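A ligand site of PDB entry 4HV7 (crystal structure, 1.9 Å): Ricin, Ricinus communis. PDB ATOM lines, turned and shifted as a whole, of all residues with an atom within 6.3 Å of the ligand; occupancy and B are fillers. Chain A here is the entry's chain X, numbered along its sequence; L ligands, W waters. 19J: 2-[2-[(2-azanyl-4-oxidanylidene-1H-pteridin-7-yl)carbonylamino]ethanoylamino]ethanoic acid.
The backbone carbonyl oxygen of Gly 121 sits close to the side-chain hydroxyl of Tyr 80 (3.3 Å).
The side-chain hydroxyl (OH) of Tyr 123 sits at hydrogen-bond distance from the side-chain carboxylate (OE2) of Glu 177 (2.6 Å).
NH2 of Arg 180 sits at hydrogen-bond distance from O of Asn 78 (2.8 Å).
OH of Tyr 80 lies within hydrogen-bond range of OD1 of Asn 122 (3.0 Å).
OD1 of Asn 78 sits close to N of Tyr 80, 3.1 Å away.
O of Ile 172 lies within hydrogen-bond range of N of Glu 177 (3.0 Å).
OG of Ser 176 lies within hydrogen-bond range of O of Ala 79.
The backbone NH of Phe 93 is in hydrogen-bond range of the backbone carbonyl oxygen of Val 82 (3.1 Å).
Residues that only touch the ligand: Ile 172, Ala 79, Asn 122, Phe 93 and Glu 177.
Of the 21 residues printed, 11 come within 4 Å of the ligand.
The backbone carbonyl oxygen (O) of Gly 121 is in hydrogen-bond range of a nitrogen (N1) of the ligand (3.2 Å).
N2 of the ligand sits at hydrogen-bond distance from N of Val 81, at 3.0 Å.
O of Val 81 lies within hydrogen-bond range of N1 of the ligand (2.8 Å).
The backbone NH of Tyr 123 sits at hydrogen-bond distance from an oxygen (O2) of the ligand, at 2.9 Å.
An oxygen (O1) of the ligand lies within hydrogen-bond range of the guanidinium group (NH2) of Arg 180 (2.9 Å).
OH of Tyr 80 lies close to N3 of the ligand (3.4 Å).
An oxygen (O1) of the ligand sits close to the side-chain hydroxyl (OG) of Ser 176 (3.4 Å).
Water W2 lies within hydrogen-bond range of the backbone carbonyl oxygen (O) of Asn 209 (2.7 Å) and an oxygen (O3) of the ligand (2.8 Å).
Water W1 lies within hydrogen-bond range of an oxygen (O2) of the ligand (2.9 Å), the backbone NH of Asp 124 (2.9 Å) and the backbone NH of Tyr 123 (3.4 Å).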
ATOM      1  N   ASN A  78     -29.898  21.571 -17.821  1.00  0.00           N
ATOM      2  CA  ASN A  78     -30.279  20.285 -18.409  1.00  0.00           C
ATOM      3  C   ASN A  78     -29.637  19.057 -17.747  1.00  0.00           C
ATOM      4  O   ASN A  78     -29.862  17.930 -18.187  1.00  0.00           O
ATOM      5  CB  ASN A  78     -29.992  20.275 -19.919  1.00  0.00           C
ATOM      6  CG  ASN A  78     -28.551  20.648 -20.231  1.00  0.00           C
ATOM      7  OD1 ASN A  78     -27.704  20.735 -19.338  1.00  0.00           O
ATOM      8  ND2 ASN A  78     -28.263  20.861 -21.519  1.00  0.00           N
ATOM      9  N   ALA A  79     -28.873  19.284 -16.682  1.00  0.00           N
ATOM     10  CA  ALA A  79     -28.181  18.211 -15.947  1.00  0.00           C
ATOM     11  C   ALA A  79     -27.069  17.563 -16.786  1.00  0.00           C
ATOM     12  O   ALA A  79     -26.526  16.509 -16.415  1.00  0.00           O
ATOM     13  CB  ALA A  79     -29.187  17.166 -15.440  1.00  0.00           C
ATOM     14  N   TYR A  80     -26.707  18.227 -17.874  1.00  0.00           N
ATOM     15  CA  TYR A  80     -25.727  17.729 -18.842  1.00  0.00           C
ATOM     16  C   TYR A  80     -24.303  17.769 -18.276  1.00  0.00           C
ATOM     17  O   TYR A  80     -23.908  18.776 -17.680  1.00  0.00           O
ATOM     18  CB  TYR A  80     -25.824  18.597 -20.095  1.00  0.00           C
ATOM     19  CG  TYR A  80     -25.159  18.045 -21.340  1.00  0.00           C
ATOM     20  CD1 TYR A  80     -25.878  17.311 -22.261  1.00  0.00           C
ATOM     21  CD2 TYR A  80     -23.823  18.287 -21.588  1.00  0.00           C
ATOM     22  CE1 TYR A  80     -25.285  16.822 -23.402  1.00  0.00           C
ATOM     23  CE2 TYR A  80     -23.207  17.805 -22.734  1.00  0.00           C
ATOM     24  CZ  TYR A  80     -23.945  17.064 -23.635  1.00  0.00           C
ATOM     25  OH  TYR A  80     -23.352  16.575 -24.776  1.00  0.00           O
ATOM     26  N   VAL A  81     -23.554  16.686 -18.439  1.00  0.00           N
ATOM     27  CA  VAL A  81     -22.147  16.678 -18.050  1.00  0.00           C
ATOM     28  C   VAL A  81     -21.388  17.423 -19.138  1.00  0.00           C
ATOM     29  O   VAL A  81     -21.311  16.943 -20.272  1.00  0.00           O
ATOM     30  CB  VAL A  81     -21.599  15.254 -17.936  1.00  0.00           C
ATOM     31  CG1 VAL A  81     -20.096  15.279 -17.646  1.00  0.00           C
ATOM     32  CG2 VAL A  81     -22.344  14.452 -16.843  1.00  0.00           C
ATOM     33  N   VAL A  82     -20.823  18.586 -18.821  1.00  0.00           N
ATOM     34  CA  VAL A  82     -20.163  19.414 -19.856  1.00  0.00           C
ATOM     35  C   VAL A  82     -18.644  19.265 -19.917  1.00  0.00           C
ATOM     36  O   VAL A  82     -18.001  19.733 -20.868  1.00  0.00           O
ATOM     37  CB  VAL A  82     -20.474  20.910 -19.681  1.00  0.00           C
ATOM     38  CG1 VAL A  82     -21.978  21.161 -19.743  1.00  0.00           C
ATOM     39  CG2 VAL A  82     -19.891  21.413 -18.371  1.00  0.00           C
ATOM     40  N   PHE A  93     -16.428  19.073 -23.435  1.00  0.00           N
ATOM     41  CA  PHE A  93     -16.997  18.688 -24.721  1.00  0.00           C
ATOM     42  C   PHE A  93     -17.155  19.916 -25.623  1.00  0.00           C
ATOM     43  O   PHE A  93     -17.230  21.055 -25.136  1.00  0.00           O
ATOM     44  CB  PHE A  93     -18.354  17.991 -24.540  1.00  0.00           C
ATOM     45  CG  PHE A  93     -18.280  16.682 -23.820  1.00  0.00           C
ATOM     46  CD1 PHE A  93     -17.648  15.587 -24.398  1.00  0.00           C
ATOM     47  CD2 PHE A  93     -18.881  16.528 -22.564  1.00  0.00           C
ATOM     48  CE1 PHE A  93     -17.593  14.366 -23.748  1.00  0.00           C
ATOM     49  CE2 PHE A  93     -18.822  15.308 -21.900  1.00  0.00           C
ATOM     50  CZ  PHE A  93     -18.176  14.230 -22.489  1.00  0.00           C
ATOM     51  N   GLY A 121     -20.720  15.960 -26.633  1.00  0.00           N
ATOM     52  CA  GLY A 121     -20.877  14.956 -25.605  1.00  0.00           C
ATOM     53  C   GLY A 121     -22.183  14.165 -25.611  1.00  0.00           C
ATOM     54  O   GLY A 121     -22.466  13.448 -24.658  1.00  0.00           O
ATOM     55  N   ASN A 122     -22.968  14.288 -26.677  1.00  0.00           N
ATOM     56  CA  ASN A 122     -24.217  13.543 -26.785  1.00  0.00           C
ATOM     57  C   ASN A 122     -23.973  12.036 -26.906  1.00  0.00           C
ATOM     58  O   ASN A 122     -22.906  11.619 -27.373  1.00  0.00           O
ATOM     59  CB  ASN A 122     -25.044  14.024 -27.992  1.00  0.00           C
ATOM     60  CG  ASN A 122     -25.739  15.359 -27.739  1.00  0.00           C
ATOM     61  OD1 ASN A 122     -25.543  15.997 -26.691  1.00  0.00           O
ATOM     62  ND2 ASN A 122     -26.543  15.797 -28.704  1.00  0.00           N
ATOM     63  N   TYR A 123     -24.952  11.224 -26.527  1.00  0.00           N
ATOM     64  CA  TYR A 123     -24.791   9.766 -26.571  1.00  0.00           C
ATOM     65  C   TYR A 123     -24.359   9.310 -27.970  1.00  0.00           C
ATOM     66  O   TYR A 123     -23.460   8.481 -28.102  1.00  0.00           O
ATOM     67  CB  TYR A 123     -26.086   9.047 -26.194  1.00  0.00           C
ATOM     68  CG  TYR A 123     -26.438   9.082 -24.719  1.00  0.00           C
ATOM     69  CD1 TYR A 123     -25.470   8.891 -23.742  1.00  0.00           C
ATOM     70  CD2 TYR A 123     -27.750   9.302 -24.318  1.00  0.00           C
ATOM     71  CE1 TYR A 123     -25.809   8.918 -22.381  1.00  0.00           C
ATOM     72  CE2 TYR A 123     -28.097   9.322 -22.977  1.00  0.00           C
ATOM     73  CZ  TYR A 123     -27.119   9.136 -22.009  1.00  0.00           C
ATOM     74  OH  TYR A 123     -27.469   9.155 -20.681  1.00  0.00           O
ATOM     75  N   ASP A 124     -25.011   9.827 -29.003  1.00  0.00           N
ATOM     76  CA  ASP A 124     -24.726   9.348 -30.351  1.00  0.00           C
ATOM     77  C   ASP A 124     -23.238   9.446 -30.663  1.00  0.00           C
ATOM     78  O   ASP A 124     -22.635   8.469 -31.126  1.00  0.00           O
ATOM     79  CB  ASP A 124     -25.568  10.104 -31.384  1.00  0.00           C
ATOM     80  CG  ASP A 124     -25.429   9.519 -32.780  1.00  0.00           C
ATOM     81  OD1 ASP A 124     -24.790   8.450 -32.922  1.00  0.00           O
ATOM     82  OD2 ASP A 124     -25.969  10.112 -33.727  1.00  0.00           O
ATOM     83  N   LEU A 126     -20.707   9.848 -28.443  1.00  0.00           N
ATOM     84  CA  LEU A 126     -19.897   9.071 -27.511  1.00  0.00           C
ATOM     85  C   LEU A 126     -19.920   7.582 -27.857  1.00  0.00           C
ATOM     86  O   LEU A 126     -18.889   6.905 -27.755  1.00  0.00           O
ATOM     87  CB  LEU A 126     -20.369   9.313 -26.061  1.00  0.00           C
ATOM     88  CG  LEU A 126     -20.071  10.701 -25.468  1.00  0.00           C
ATOM     89  CD1 LEU A 126     -20.561  10.769 -24.026  1.00  0.00           C
ATOM     90  CD2 LEU A 126     -18.575  11.028 -25.539  1.00  0.00           C
ATOM     91  N   ARG A 134     -25.043   2.175 -25.806  1.00  0.00           N
ATOM     92  CA  ARG A 134     -25.449   2.108 -24.411  1.00  0.00           C
ATOM     93  C   ARG A 134     -25.942   0.705 -24.057  1.00  0.00           C
ATOM     94  O   ARG A 134     -25.611   0.175 -22.986  1.00  0.00           O
ATOM     95  CB  ARG A 134     -26.543   3.135 -24.117  1.00  0.00           C
ATOM     96  CG  ARG A 134     -26.006   4.542 -23.987  1.00  0.00           C
ATOM     97  CD  ARG A 134     -27.162   5.565 -23.939  1.00  0.00           C
ATOM     98  NE  ARG A 134     -27.697   5.820 -25.275  1.00  0.00           N
ATOM     99  CZ  ARG A 134     -28.922   6.284 -25.521  1.00  0.00           C
ATOM    100  NH1 ARG A 134     -29.756   6.547 -24.512  1.00  0.00           N
ATOM    101  NH2 ARG A 134     -29.310   6.493 -26.769  1.00  0.00           N
ATOM    102  N   ILE A 172     -22.473   9.561 -17.101  1.00  0.00           N
ATOM    103  CA  ILE A 172     -23.678  10.321 -17.459  1.00  0.00           C
ATOM    104  C   ILE A 172     -24.933   9.580 -17.019  1.00  0.00           C
ATOM    105  O   ILE A 172     -25.831  10.162 -16.453  1.00  0.00           O
ATOM    106  CB  ILE A 172     -23.729  10.604 -18.983  1.00  0.00           C
ATOM    107  CG1 ILE A 172     -22.530  11.507 -19.391  1.00  0.00           C
ATOM    108  CG2 ILE A 172     -25.086  11.166 -19.416  1.00  0.00           C
ATOM    109  CD1 ILE A 172     -22.258  11.474 -20.881  1.00  0.00           C
ATOM    110  N   SER A 176     -26.332  11.887 -14.198  1.00  0.00           N
ATOM    111  CA  SER A 176     -27.349  12.731 -14.832  1.00  0.00           C
ATOM    112  C   SER A 176     -28.683  12.023 -15.072  1.00  0.00           C
ATOM    113  O   SER A 176     -29.744  12.569 -14.719  1.00  0.00           O
ATOM    114  CB  SER A 176     -26.815  13.302 -16.152  1.00  0.00           C
ATOM    115  OG  SER A 176     -25.596  13.995 -15.918  1.00  0.00           O
ATOM    116  N   GLU A 177     -28.663  10.826 -15.654  1.00  0.00           N
ATOM    117  CA  GLU A 177     -29.927  10.135 -15.942  1.00  0.00           C
ATOM    118  C   GLU A 177     -30.631   9.696 -14.661  1.00  0.00           C
ATOM    119  O   GLU A 177     -31.861   9.759 -14.541  1.00  0.00           O
ATOM    120  CB  GLU A 177     -29.745   8.946 -16.892  1.00  0.00           C
ATOM    121  CG  GLU A 177     -29.159   9.288 -18.250  1.00  0.00           C
ATOM    122  CD  GLU A 177     -30.104  10.066 -19.164  1.00  0.00           C
ATOM    123  OE1 GLU A 177     -31.171  10.513 -18.698  1.00  0.00           O
ATOM    124  OE2 GLU A 177     -29.768  10.228 -20.360  1.00  0.00           O
ATOM    125  N   ARG A 180     -32.355  12.672 -13.295  1.00  0.00           N
ATOM    126  CA  ARG A 180     -33.559  12.986 -14.083  1.00  0.00           C
ATOM    127  C   ARG A 180     -34.748  12.044 -13.802  1.00  0.00           C
ATOM    128  O   ARG A 180     -35.918  12.476 -13.821  1.00  0.00           O
ATOM    129  CB  ARG A 180     -33.259  12.950 -15.589  1.00  0.00           C
ATOM    130  CG  ARG A 180     -32.324  14.050 -16.064  1.00  0.00           C
ATOM    131  CD  ARG A 180     -31.896  13.777 -17.516  1.00  0.00           C
ATOM    132  NE  ARG A 180     -30.931  14.762 -18.012  1.00  0.00           N
ATOM    133  CZ  ARG A 180     -29.800  14.434 -18.649  1.00  0.00           C
ATOM    134  NH1 ARG A 180     -29.509  13.164 -18.868  1.00  0.00           N
ATOM    135  NH2 ARG A 180     -28.981  15.389 -19.085  1.00  0.00           N
ATOM    136  N   GLU A 208     -34.319   7.451 -21.377  1.00  0.00           N
ATOM    137  CA  GLU A 208     -33.188   8.345 -21.650  1.00  0.00           C
ATOM    138  C   GLU A 208     -33.428   9.107 -22.938  1.00  0.00           C
ATOM    139  O   GLU A 208     -33.290  10.333 -22.988  1.00  0.00           O
ATOM    140  CB  GLU A 208     -31.876   7.558 -21.748  1.00  0.00           C
ATOM    141  CG  GLU A 208     -31.362   6.989 -20.409  1.00  0.00           C
ATOM    142  CD  GLU A 208     -30.147   6.116 -20.561  1.00  0.00           C
ATOM    143  OE1 GLU A 208     -29.699   5.904 -21.707  1.00  0.00           O
ATOM    144  OE2 GLU A 208     -29.621   5.634 -19.518  1.00  0.00           O
ATOM    145  N   ASN A 209     -33.787   8.378 -23.994  1.00  0.00           N
ATOM    146  CA  ASN A 209     -34.018   8.987 -25.296  1.00  0.00           C
ATOM    147  C   ASN A 209     -35.207   9.945 -25.334  1.00  0.00           C
ATOM    148  O   ASN A 209     -35.250  10.837 -26.178  1.00  0.00           O
ATOM    149  CB  ASN A 209     -34.207   7.912 -26.367  1.00  0.00           C
ATOM    150  CG  ASN A 209     -32.948   7.086 -26.582  1.00  0.00           C
ATOM    151  OD1 ASN A 209     -31.833   7.553 -26.325  1.00  0.00           O
ATOM    152  ND2 ASN A 209     -33.118   5.875 -27.079  1.00  0.00           N
ATOM    153  N   TRP A 211     -36.484  11.879 -22.727  1.00  0.00           N
ATOM    154  CA  TRP A 211     -36.535  12.902 -21.675  1.00  0.00           C
ATOM    155  C   TRP A 211     -37.001  14.259 -22.202  1.00  0.00           C
ATOM    156  O   TRP A 211     -37.883  14.881 -21.625  1.00  0.00           O
ATOM    157  CB  TRP A 211     -35.177  13.060 -20.970  1.00  0.00           C
ATOM    158  CG  TRP A 211     -35.210  14.008 -19.783  1.00  0.00           C
ATOM    159  CD1 TRP A 211     -36.003  13.909 -18.676  1.00  0.00           C
ATOM    160  CD2 TRP A 211     -34.368  15.162 -19.565  1.00  0.00           C
ATOM    161  NE1 TRP A 211     -35.727  14.930 -17.795  1.00  0.00           N
ATOM    162  CE2 TRP A 211     -34.741  15.711 -18.321  1.00  0.00           C
ATOM    163  CE3 TRP A 211     -33.366  15.774 -20.318  1.00  0.00           C
ATOM    164  CZ2 TRP A 211     -34.110  16.858 -17.801  1.00  0.00           C
ATOM    165  CZ3 TRP A 211     -32.757  16.920 -19.800  1.00  0.00           C
ATOM    166  CH2 TRP A 211     -33.126  17.446 -18.549  1.00  0.00           C
ATOM    167  N   GLY A 212     -36.406  14.721 -23.294  1.00  0.00           N
ATOM    168  CA  GLY A 212     -36.796  16.012 -23.861  1.00  0.00           C
ATOM    169  C   GLY A 212     -38.253  16.039 -24.303  1.00  0.00           C
ATOM    170  O   GLY A 212     -38.987  17.004 -24.004  1.00  0.00           O
ATOM    171  N   ARG A 258     -39.129  24.048 -20.800  1.00  0.00           N
ATOM    172  CA  ARG A 258     -39.528  24.275 -22.206  1.00  0.00           C
ATOM    173  C   ARG A 258     -40.381  25.522 -22.385  1.00  0.00           C
ATOM    174  O   ARG A 258     -40.078  26.371 -23.221  1.00  0.00           O
ATOM    175  CB  ARG A 258     -40.328  23.091 -22.740  1.00  0.00           C
ATOM    176  CG  ARG A 258     -39.582  21.816 -22.738  1.00  0.00           C
ATOM    177  CD  ARG A 258     -38.334  21.966 -23.523  1.00  0.00           C
ATOM    178  NE  ARG A 258     -38.028  20.726 -24.205  1.00  0.00           N
ATOM    179  CZ  ARG A 258     -36.823  20.344 -24.554  1.00  0.00           C
ATOM    180  NH1 ARG A 258     -35.771  21.110 -24.265  1.00  0.00           N
ATOM    181  NH2 ARG A 258     -36.670  19.189 -25.184  1.00  0.00           N
HETATM  182  C1  19J L   1     -23.747  14.456 -21.704  1.00  0.00           C
HETATM  183  N1  19J L   1     -22.440  14.813 -21.786  1.00  0.00           N
HETATM  184  O1  19J L   1     -26.271  14.411 -19.235  1.00  0.00           O
HETATM  185  C2  19J L   1     -25.684  14.279 -20.329  1.00  0.00           C
HETATM  186  N2  19J L   1     -24.391  14.631 -20.509  1.00  0.00           N
HETATM  187  C3  19J L   1     -26.403  13.752 -21.494  1.00  0.00           C
HETATM  188  N3  19J L   1     -24.360  13.969 -22.803  1.00  0.00           N
HETATM  189  O2  19J L   1     -27.635  12.091 -25.982  1.00  0.00           O
HETATM  190  C4  19J L   1     -25.661  13.622 -22.752  1.00  0.00           C
HETATM  191  N4  19J L   1     -26.298  13.137 -23.822  1.00  0.00           N
HETATM  192  C5  19J L   1     -27.602  12.787 -23.734  1.00  0.00           C
HETATM  193  N5  19J L   1     -27.705  13.392 -21.429  1.00  0.00           N
HETATM  194  C6  19J L   1     -28.294  12.918 -22.540  1.00  0.00           C
HETATM  195  C7  19J L   1     -28.284  12.294 -24.975  1.00  0.00           C
HETATM  196  N6  19J L   1     -29.604  12.185 -24.982  1.00  0.00           N
HETATM  197  C8  19J L   1     -30.352  11.881 -26.181  1.00  0.00           C
HETATM  198  C9  19J L   1     -30.432  13.006 -27.195  1.00  0.00           C
HETATM  199  O3  19J L   1     -30.804  12.773 -28.337  1.00  0.00           O
HETATM  200  N7  19J L   1     -30.088  14.239 -26.816  1.00  0.00           N
HETATM  201  C10 19J L   1     -30.343  15.393 -27.655  1.00  0.00           C
HETATM  202  C11 19J L   1     -31.794  15.829 -27.632  1.00  0.00           C
HETATM  203  O5  19J L   1     -32.105  16.938 -27.224  1.00  0.00           O
HETATM  204  O4  19J L   1     -32.768  15.003 -28.049  1.00  0.00           O
HETATM  205  O   HOH W   1     -27.436  11.472 -28.800  1.00  0.00           O
HETATM  206  O   HOH W   2     -33.351  11.648 -27.891  1.00  0.00           O
HETATM  207  O   HOH W   3     -31.601  13.733 -23.258  1.00  0.00           O
